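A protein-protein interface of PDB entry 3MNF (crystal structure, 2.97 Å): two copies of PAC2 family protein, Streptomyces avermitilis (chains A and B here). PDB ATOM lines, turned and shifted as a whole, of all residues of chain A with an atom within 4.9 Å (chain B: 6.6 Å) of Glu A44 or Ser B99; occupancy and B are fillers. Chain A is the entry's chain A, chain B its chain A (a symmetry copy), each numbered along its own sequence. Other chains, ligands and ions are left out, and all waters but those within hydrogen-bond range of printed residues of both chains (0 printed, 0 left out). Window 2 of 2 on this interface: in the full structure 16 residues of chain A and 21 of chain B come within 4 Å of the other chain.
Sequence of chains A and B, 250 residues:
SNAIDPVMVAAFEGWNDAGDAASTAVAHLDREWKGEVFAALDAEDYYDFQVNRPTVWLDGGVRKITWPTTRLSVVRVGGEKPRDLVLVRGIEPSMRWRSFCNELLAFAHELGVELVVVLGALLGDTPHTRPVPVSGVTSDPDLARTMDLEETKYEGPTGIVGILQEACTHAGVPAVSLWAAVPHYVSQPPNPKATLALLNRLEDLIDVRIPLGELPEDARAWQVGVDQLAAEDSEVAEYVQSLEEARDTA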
ATOM      1  N   ASP A  42      15.034  14.461  -6.796  1.00  0.00           N
ATOM      2  CA  ASP A  42      14.824  13.382  -7.733  1.00  0.00           C
ATOM      3  C   ASP A  42      14.455  13.900  -9.130  1.00  0.00           C
ATOM      4  O   ASP A  42      13.312  14.299  -9.366  1.00  0.00           O
ATOM      5  CB  ASP A  42      13.701  12.510  -7.204  1.00  0.00           C
ATOM      6  CG  ASP A  42      13.548  11.257  -7.979  1.00  0.00           C
ATOM      7  OD1 ASP A  42      13.978  11.272  -9.144  1.00  0.00           O
ATOM      8  OD2 ASP A  42      13.023  10.261  -7.426  1.00  0.00           O
ATOM      9  N   ALA A  43      15.407  13.854 -10.060  1.00  0.00           N
ATOM     10  CA  ALA A  43      15.208  14.373 -11.403  1.00  0.00           C
ATOM     11  C   ALA A  43      13.968  13.805 -12.049  1.00  0.00           C
ATOM     12  O   ALA A  43      13.212  14.531 -12.687  1.00  0.00           O
ATOM     13  CB  ALA A  43      16.389  14.099 -12.234  1.00  0.00           C
ATOM     14  N   GLU A  44      13.743  12.512 -11.848  1.00  0.00           N
ATOM     15  CA  GLU A  44      12.578  11.796 -12.362  1.00  0.00           C
ATOM     16  C   GLU A  44      11.260  12.577 -12.282  1.00  0.00           C
ATOM     17  O   GLU A  44      10.408  12.438 -13.153  1.00  0.00           O
ATOM     18  CB  GLU A  44      12.442  10.498 -11.611  1.00  0.00           C
ATOM     19  CG  GLU A  44      11.667   9.416 -12.310  1.00  0.00           C
ATOM     20  CD  GLU A  44      12.474   8.644 -13.338  1.00  0.00           C
ATOM     21  OE1 GLU A  44      13.504   9.158 -13.848  1.00  0.00           O
ATOM     22  OE2 GLU A  44      12.043   7.518 -13.653  1.00  0.00           O
ATOM     23  N   ASP A  45      11.098  13.420 -11.262  1.00  0.00           N
ATOM     24  CA  ASP A  45       9.846  14.159 -11.061  1.00  0.00           C
ATOM     25  C   ASP A  45       9.765  15.464 -11.805  1.00  0.00           C
ATOM     26  O   ASP A  45       8.671  15.997 -11.952  1.00  0.00           O
ATOM     27  CB  ASP A  45       9.594  14.442  -9.580  1.00  0.00           C
ATOM     28  CG  ASP A  45       9.262  13.174  -8.790  1.00  0.00           C
ATOM     29  OD1 ASP A  45       8.352  12.401  -9.214  1.00  0.00           O
ATOM     30  OD2 ASP A  45       9.933  12.948  -7.738  1.00  0.00           O
ATOM     31  N   TYR A  46      10.892  15.996 -12.276  1.00  0.00           N
ATOM     32  CA  TYR A  46      10.893  17.386 -12.691  1.00  0.00           C
ATOM     33  C   TYR A  46      11.403  17.728 -14.090  1.00  0.00           C
ATOM     34  O   TYR A  46      11.063  18.790 -14.644  1.00  0.00           O
ATOM     35  CB  TYR A  46      11.672  18.164 -11.671  1.00  0.00           C
ATOM     36  CG  TYR A  46      11.113  18.056 -10.277  1.00  0.00           C
ATOM     37  CD1 TYR A  46      11.864  17.513  -9.250  1.00  0.00           C
ATOM     38  CD2 TYR A  46       9.841  18.509  -9.990  1.00  0.00           C
ATOM     39  CE1 TYR A  46      11.368  17.426  -7.986  1.00  0.00           C
ATOM     40  CE2 TYR A  46       9.325  18.422  -8.713  1.00  0.00           C
ATOM     41  CZ  TYR A  46      10.097  17.883  -7.721  1.00  0.00           C
ATOM     42  OH  TYR A  46       9.586  17.797  -6.466  1.00  0.00           O
ATOM     43  N   PHE A  49      13.878  14.830 -20.232  1.00  0.00           N
ATOM     44  CA  PHE A  49      15.252  14.458 -20.471  1.00  0.00           C
ATOM     45  C   PHE A  49      15.626  14.583 -21.924  1.00  0.00           C
ATOM     46  O   PHE A  49      16.760  14.315 -22.311  1.00  0.00           O
ATOM     47  CB  PHE A  49      15.545  13.055 -19.953  1.00  0.00           C
ATOM     48  CG  PHE A  49      15.380  12.916 -18.482  1.00  0.00           C
ATOM     49  CD1 PHE A  49      16.178  13.635 -17.611  1.00  0.00           C
ATOM     50  CD2 PHE A  49      14.438  12.061 -17.958  1.00  0.00           C
ATOM     51  CE1 PHE A  49      16.026  13.504 -16.237  1.00  0.00           C
ATOM     52  CE2 PHE A  49      14.272  11.933 -16.584  1.00  0.00           C
ATOM     53  CZ  PHE A  49      15.062  12.654 -15.725  1.00  0.00           C
ATOM     54  N   MET A  95       8.785  20.654 -15.252  1.00  0.00           N
ATOM     55  CA  MET A  95       7.439  20.377 -14.749  1.00  0.00           C
ATOM     56  C   MET A  95       7.305  20.390 -13.225  1.00  0.00           C
ATOM     57  O   MET A  95       8.268  20.576 -12.517  1.00  0.00           O
ATOM     58  CB  MET A  95       6.900  19.095 -15.345  1.00  0.00           C
ATOM     59  CG  MET A  95       7.948  18.052 -15.492  1.00  0.00           C
ATOM     60  SD  MET A  95       7.380  16.455 -16.361  1.00  0.00           S
ATOM     61  CE  MET A  95       7.066  15.409 -14.735  1.00  0.00           C
ATOM     62  N   LEU B  41       4.011  -0.318 -23.027  1.00  0.00           N
ATOM     63  CA  LEU B  41       4.141   0.555 -21.868  1.00  0.00           C
ATOM     64  C   LEU B  41       3.090   1.659 -21.923  1.00  0.00           C
ATOM     65  O   LEU B  41       2.718   2.132 -23.001  1.00  0.00           O
ATOM     66  CB  LEU B  41       5.516   1.183 -21.759  1.00  0.00           C
ATOM     67  CG  LEU B  41       6.692   0.236 -21.563  1.00  0.00           C
ATOM     68  CD1 LEU B  41       7.952   1.030 -21.272  1.00  0.00           C
ATOM     69  CD2 LEU B  41       6.430  -0.730 -20.451  1.00  0.00           C
ATOM     70  N   TYR B  46       5.169   8.542 -19.857  1.00  0.00           N
ATOM     71  CA  TYR B  46       6.476   8.784 -20.438  1.00  0.00           C
ATOM     72  C   TYR B  46       6.599   9.825 -21.549  1.00  0.00           C
ATOM     73  O   TYR B  46       7.695  10.360 -21.795  1.00  0.00           O
ATOM     74  CB  TYR B  46       7.008   7.467 -20.925  1.00  0.00           C
ATOM     75  CG  TYR B  46       7.122   6.428 -19.841  1.00  0.00           C
ATOM     76  CD1 TYR B  46       6.407   5.246 -19.911  1.00  0.00           C
ATOM     77  CD2 TYR B  46       7.956   6.626 -18.758  1.00  0.00           C
ATOM     78  CE1 TYR B  46       6.518   4.297 -18.941  1.00  0.00           C
ATOM     79  CE2 TYR B  46       8.074   5.674 -17.766  1.00  0.00           C
ATOM     80  CZ  TYR B  46       7.354   4.516 -17.870  1.00  0.00           C
ATOM     81  OH  TYR B  46       7.471   3.582 -16.891  1.00  0.00           O
ATOM     82  N   MET B  95      10.152  11.636 -20.624  1.00  0.00           N
ATOM     83  CA  MET B  95      10.321  11.739 -19.174  1.00  0.00           C
ATOM     84  C   MET B  95      10.424  10.400 -18.440  1.00  0.00           C
ATOM     85  O   MET B  95      10.325   9.354 -19.039  1.00  0.00           O
ATOM     86  CB  MET B  95       9.250  12.623 -18.573  1.00  0.00           C
ATOM     87  CG  MET B  95       7.930  12.444 -19.230  1.00  0.00           C
ATOM     88  SD  MET B  95       6.561  13.619 -18.623  1.00  0.00           S
ATOM     89  CE  MET B  95       5.716  12.363 -17.380  1.00  0.00           C
ATOM     90  N   ARG B  96      10.678  10.465 -17.138  1.00  0.00           N
ATOM     91  CA  ARG B  96      10.836   9.281 -16.265  1.00  0.00           C
ATOM     92  C   ARG B  96      11.617   8.082 -16.861  1.00  0.00           C
ATOM     93  O   ARG B  96      11.178   6.924 -16.831  1.00  0.00           O
ATOM     94  CB  ARG B  96       9.480   8.889 -15.684  1.00  0.00           C
ATOM     95  CG  ARG B  96       8.638  10.101 -15.292  1.00  0.00           C
ATOM     96  CD  ARG B  96       7.247   9.716 -14.811  1.00  0.00           C
ATOM     97  NE  ARG B  96       7.363   8.633 -13.845  1.00  0.00           N
ATOM     98  CZ  ARG B  96       7.667   8.819 -12.561  1.00  0.00           C
ATOM     99  NH1 ARG B  96       7.830  10.063 -12.073  1.00  0.00           N
ATOM    100  NH2 ARG B  96       7.797   7.759 -11.757  1.00  0.00           N
ATOM    101  N   TRP B  97      12.796   8.372 -17.392  1.00  0.00           N
ATOM    102  CA  TRP B  97      13.637   7.314 -17.968  1.00  0.00           C
ATOM    103  C   TRP B  97      14.012   6.199 -16.995  1.00  0.00           C
ATOM    104  O   TRP B  97      14.106   5.047 -17.404  1.00  0.00           O
ATOM    105  CB  TRP B  97      14.909   7.902 -18.541  1.00  0.00           C
ATOM    106  CG  TRP B  97      14.698   8.735 -19.756  1.00  0.00           C
ATOM    107  CD1 TRP B  97      13.503   9.164 -20.286  1.00  0.00           C
ATOM    108  CD2 TRP B  97      15.720   9.304 -20.570  1.00  0.00           C
ATOM    109  NE1 TRP B  97      13.730   9.946 -21.385  1.00  0.00           N
ATOM    110  CE2 TRP B  97      15.082  10.048 -21.581  1.00  0.00           C
ATOM    111  CE3 TRP B  97      17.118   9.244 -20.548  1.00  0.00           C
ATOM    112  CZ2 TRP B  97      15.794  10.716 -22.570  1.00  0.00           C
ATOM    113  CZ3 TRP B  97      17.821   9.926 -21.503  1.00  0.00           C
ATOM    114  CH2 TRP B  97      17.163  10.656 -22.507  1.00  0.00           C
ATOM    115  N   ARG B  98      14.249   6.538 -15.720  1.00  0.00           N
ATOM    116  CA  ARG B  98      14.575   5.530 -14.726  1.00  0.00           C
ATOM    117  C   ARG B  98      13.440   4.513 -14.528  1.00  0.00           C
ATOM    118  O   ARG B  98      13.694   3.321 -14.402  1.00  0.00           O
ATOM    119  CB  ARG B  98      15.028   6.168 -13.418  1.00  0.00           C
ATOM    120  CG  ARG B  98      15.074   5.202 -12.222  1.00  0.00           C
ATOM    121  CD  ARG B  98      15.755   5.766 -10.988  1.00  0.00           C
ATOM    122  NE  ARG B  98      15.306   7.097 -10.518  1.00  0.00           N
ATOM    123  CZ  ARG B  98      14.182   7.351  -9.840  1.00  0.00           C
ATOM    124  NH1 ARG B  98      13.307   6.388  -9.565  1.00  0.00           N
ATOM    125  NH2 ARG B  98      13.921   8.584  -9.439  1.00  0.00           N
ATOM    126  N   SER B  99      12.199   4.979 -14.540  1.00  0.00           N
ATOM    127  CA  SER B  99      11.044   4.111 -14.406  1.00  0.00           C
ATOM    128  C   SER B  99      10.848   3.344 -15.685  1.00  0.00           C
ATOM    129  O   SER B  99      10.558   2.153 -15.661  1.00  0.00           O
ATOM    130  CB  SER B  99       9.801   4.929 -14.156  1.00  0.00           C
ATOM    131  OG  SER B  99      10.100   5.985 -13.249  1.00  0.00           O
ATOM    132  N   PHE B 100      11.000   4.027 -16.813  1.00  0.00           N
ATOM    133  CA  PHE B 100      10.852   3.410 -18.109  1.00  0.00           C
ATOM    134  C   PHE B 100      11.725   2.180 -18.166  1.00  0.00           C
ATOM    135  O   PHE B 100      11.276   1.087 -18.543  1.00  0.00           O
ATOM    136  CB  PHE B 100      11.316   4.410 -19.129  1.00  0.00           C
ATOM    137  CG  PHE B 100      11.136   3.983 -20.545  1.00  0.00           C
ATOM    138  CD1 PHE B 100       9.934   4.214 -21.204  1.00  0.00           C
ATOM    139  CD2 PHE B 100      12.202   3.433 -21.255  1.00  0.00           C
ATOM    140  CE1 PHE B 100       9.782   3.866 -22.539  1.00  0.00           C
ATOM    141  CE2 PHE B 100      12.063   3.071 -22.606  1.00  0.00           C
ATOM    142  CZ  PHE B 100      10.862   3.285 -23.246  1.00  0.00           C
ATOM    143  N   CYS B 101      12.981   2.359 -17.763  1.00  0.00           N
ATOM    144  CA  CYS B 101      13.965   1.310 -17.846  1.00  0.00           C
ATOM    145  C   CYS B 101      13.683   0.208 -16.874  1.00  0.00           C
ATOM    146  O   CYS B 101      13.873  -0.957 -17.219  1.00  0.00           O
ATOM    147  CB  CYS B 101      15.340   1.870 -17.621  1.00  0.00           C
ATOM    148  SG  CYS B 101      15.880   2.736 -19.078  1.00  0.00           S
ATOM    149  N   ASN B 102      13.220   0.565 -15.674  1.00  0.00           N
ATOM    150  CA  ASN B 102      12.803  -0.415 -14.697  1.00  0.00           C
ATOM    151  C   ASN B 102      11.669  -1.244 -15.231  1.00  0.00           C
ATOM    152  O   ASN B 102      11.634  -2.439 -15.034  1.00  0.00           O
ATOM    153  CB  ASN B 102      12.397   0.259 -13.408  1.00  0.00           C
ATOM    154  CG  ASN B 102      13.596   0.731 -12.596  1.00  0.00           C
ATOM    155  OD1 ASN B 102      14.759   0.390 -12.898  1.00  0.00           O
ATOM    156  ND2 ASN B 102      13.325   1.530 -11.544  1.00  0.00           N
ATOM    157  N   GLU B 103      10.752  -0.613 -15.950  1.00  0.00           N
ATOM    158  CA  GLU B 103       9.598  -1.316 -16.487  1.00  0.00           C
ATOM    159  C   GLU B 103      10.050  -2.395 -17.481  1.00  0.00           C
ATOM    160  O   GLU B 103       9.582  -3.530 -17.426  1.00  0.00           O
ATOM    161  CB  GLU B 103       8.603  -0.334 -17.101  1.00  0.00           C
ATOM    162  CG  GLU B 103       7.161  -0.811 -17.082  1.00  0.00           C
ATOM    163  CD  GLU B 103       6.152   0.333 -17.020  1.00  0.00           C
ATOM    164  OE1 GLU B 103       6.305   1.189 -16.145  1.00  0.00           O
ATOM    165  OE2 GLU B 103       5.196   0.401 -17.834  1.00  0.00           O
ATOM    166  N   LEU B 104      10.980  -2.054 -18.371  1.00  0.00           N
ATOM    167  CA  LEU B 104      11.497  -3.035 -19.312  1.00  0.00           C
ATOM    168  C   LEU B 104      12.244  -4.136 -18.565  1.00  0.00           C
ATOM    169  O   LEU B 104      12.036  -5.316 -18.831  1.00  0.00           O
ATOM    170  CB  LEU B 104      12.376  -2.355 -20.355  1.00  0.00           C
ATOM    171  CG  LEU B 104      11.681  -1.307 -21.248  1.00  0.00           C
ATOM    172  CD1 LEU B 104      12.672  -0.596 -22.158  1.00  0.00           C
ATOM    173  CD2 LEU B 104      10.604  -1.937 -22.085  1.00  0.00           C
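Trp B97 touches Glu A44 (N to OE1, 3.7 Å).
Phe A49 touches Arg B96 (CE2 to N, 3.9 Å).
Trp B97 touches Phe A49 (CE2 to CB, 3.5 Å).
Glu A44 touches just these residues of chain B: Arg B96 (3.3 Å), Trp B97 (3.7 Å), Arg B98 (3.2 Å) and Ser B99 (2.5 Å).
Printed residues of chain B within 4 Å of Asp A45: Arg B96 (3.7 Å).
Of the printed residues of chain B, Phe A49 touches Arg B96 (3.9 Å) and Trp B97 (3.5 Å).
Leu B41 touches none of the printed residues of chain A.
Printed residues of chain A within 4 Å of Trp B97: Glu A44 and Phe A49.
Printed residues of chain A within 4 Å of Arg B98: Asp A42 (2.7 Å) and Glu A44 (3.2 Å).
Ser B99 touches just one residue of chain A: Glu A44 (2.5 Å).
Glu B103 touches none of the printed residues of chain A.
Met A95 touches its own counterpart, Met B95.
2 positions are printed for both chains.
Of the 9 pairs that touch across the chains among the printed residues, 1 has its exchanged pair printed and touching as well.
Printed residues of chain A that touch a printed residue of chain B: Asp A42, Glu A44, Asp A45, Phe A49 and Met A95.
Of the 12 printed residues of chain B, 5 touch a printed residue of chain A.
Hydrophobic or aromatic side chains of chain B within 4 Å of the printed part of chain A: Met B95 and Trp B97.
Among the printed residues, 9 pairs touch across the chains.
The guanidinium group (NH2) of Arg B98 lies within salt-bridge range of the side-chain carboxylate (OD1) of Asp A42, at 2.7 Å.
OE2 of Glu A44 sits at hydrogen-bond distance from N of Arg B98 (3.2 Å).
The side-chain hydroxyl (OG) of Ser B99 is in hydrogen-bond range of the side-chain carboxylate (OE2) of Glu A44 (2.5 Å).
The side-chain carboxylate (OD1) of Asp A45 lies within salt-bridge range of the guanidinium group (NH1) of Arg B96.
The backbone carbonyl oxygen of Arg B96 sits close to the side-chain carboxylate of Glu A44, at 3.3 Å.
SD of Met A95 sits close to SD of Met B95.
The side-chain carboxylate (OD1) of Asp A42 sits at hydrogen-bond distance from the backbone NH (N) of Glu A44 (3.0 Å).
The backbone carbonyl oxygen of Tyr A46 sits at hydrogen-bond distance from the backbone NH of Met A95 (3.0 Å).
N of Met B95 is in hydrogen-bond range of O of Tyr B46 (3.0 Å).
The side-chain hydroxyl of Ser B99 lies within hydrogen-bond range of the guanidinium group of Arg B96, 3.3 Å away.
O of Trp B97 sits at hydrogen-bond distance from SG of Cys B101 (3.4 Å).
The backbone carbonyl oxygen (O) of Arg B98 sits close to the side-chain amide nitrogen (ND2) of Asn B102, 3.4 Å away.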
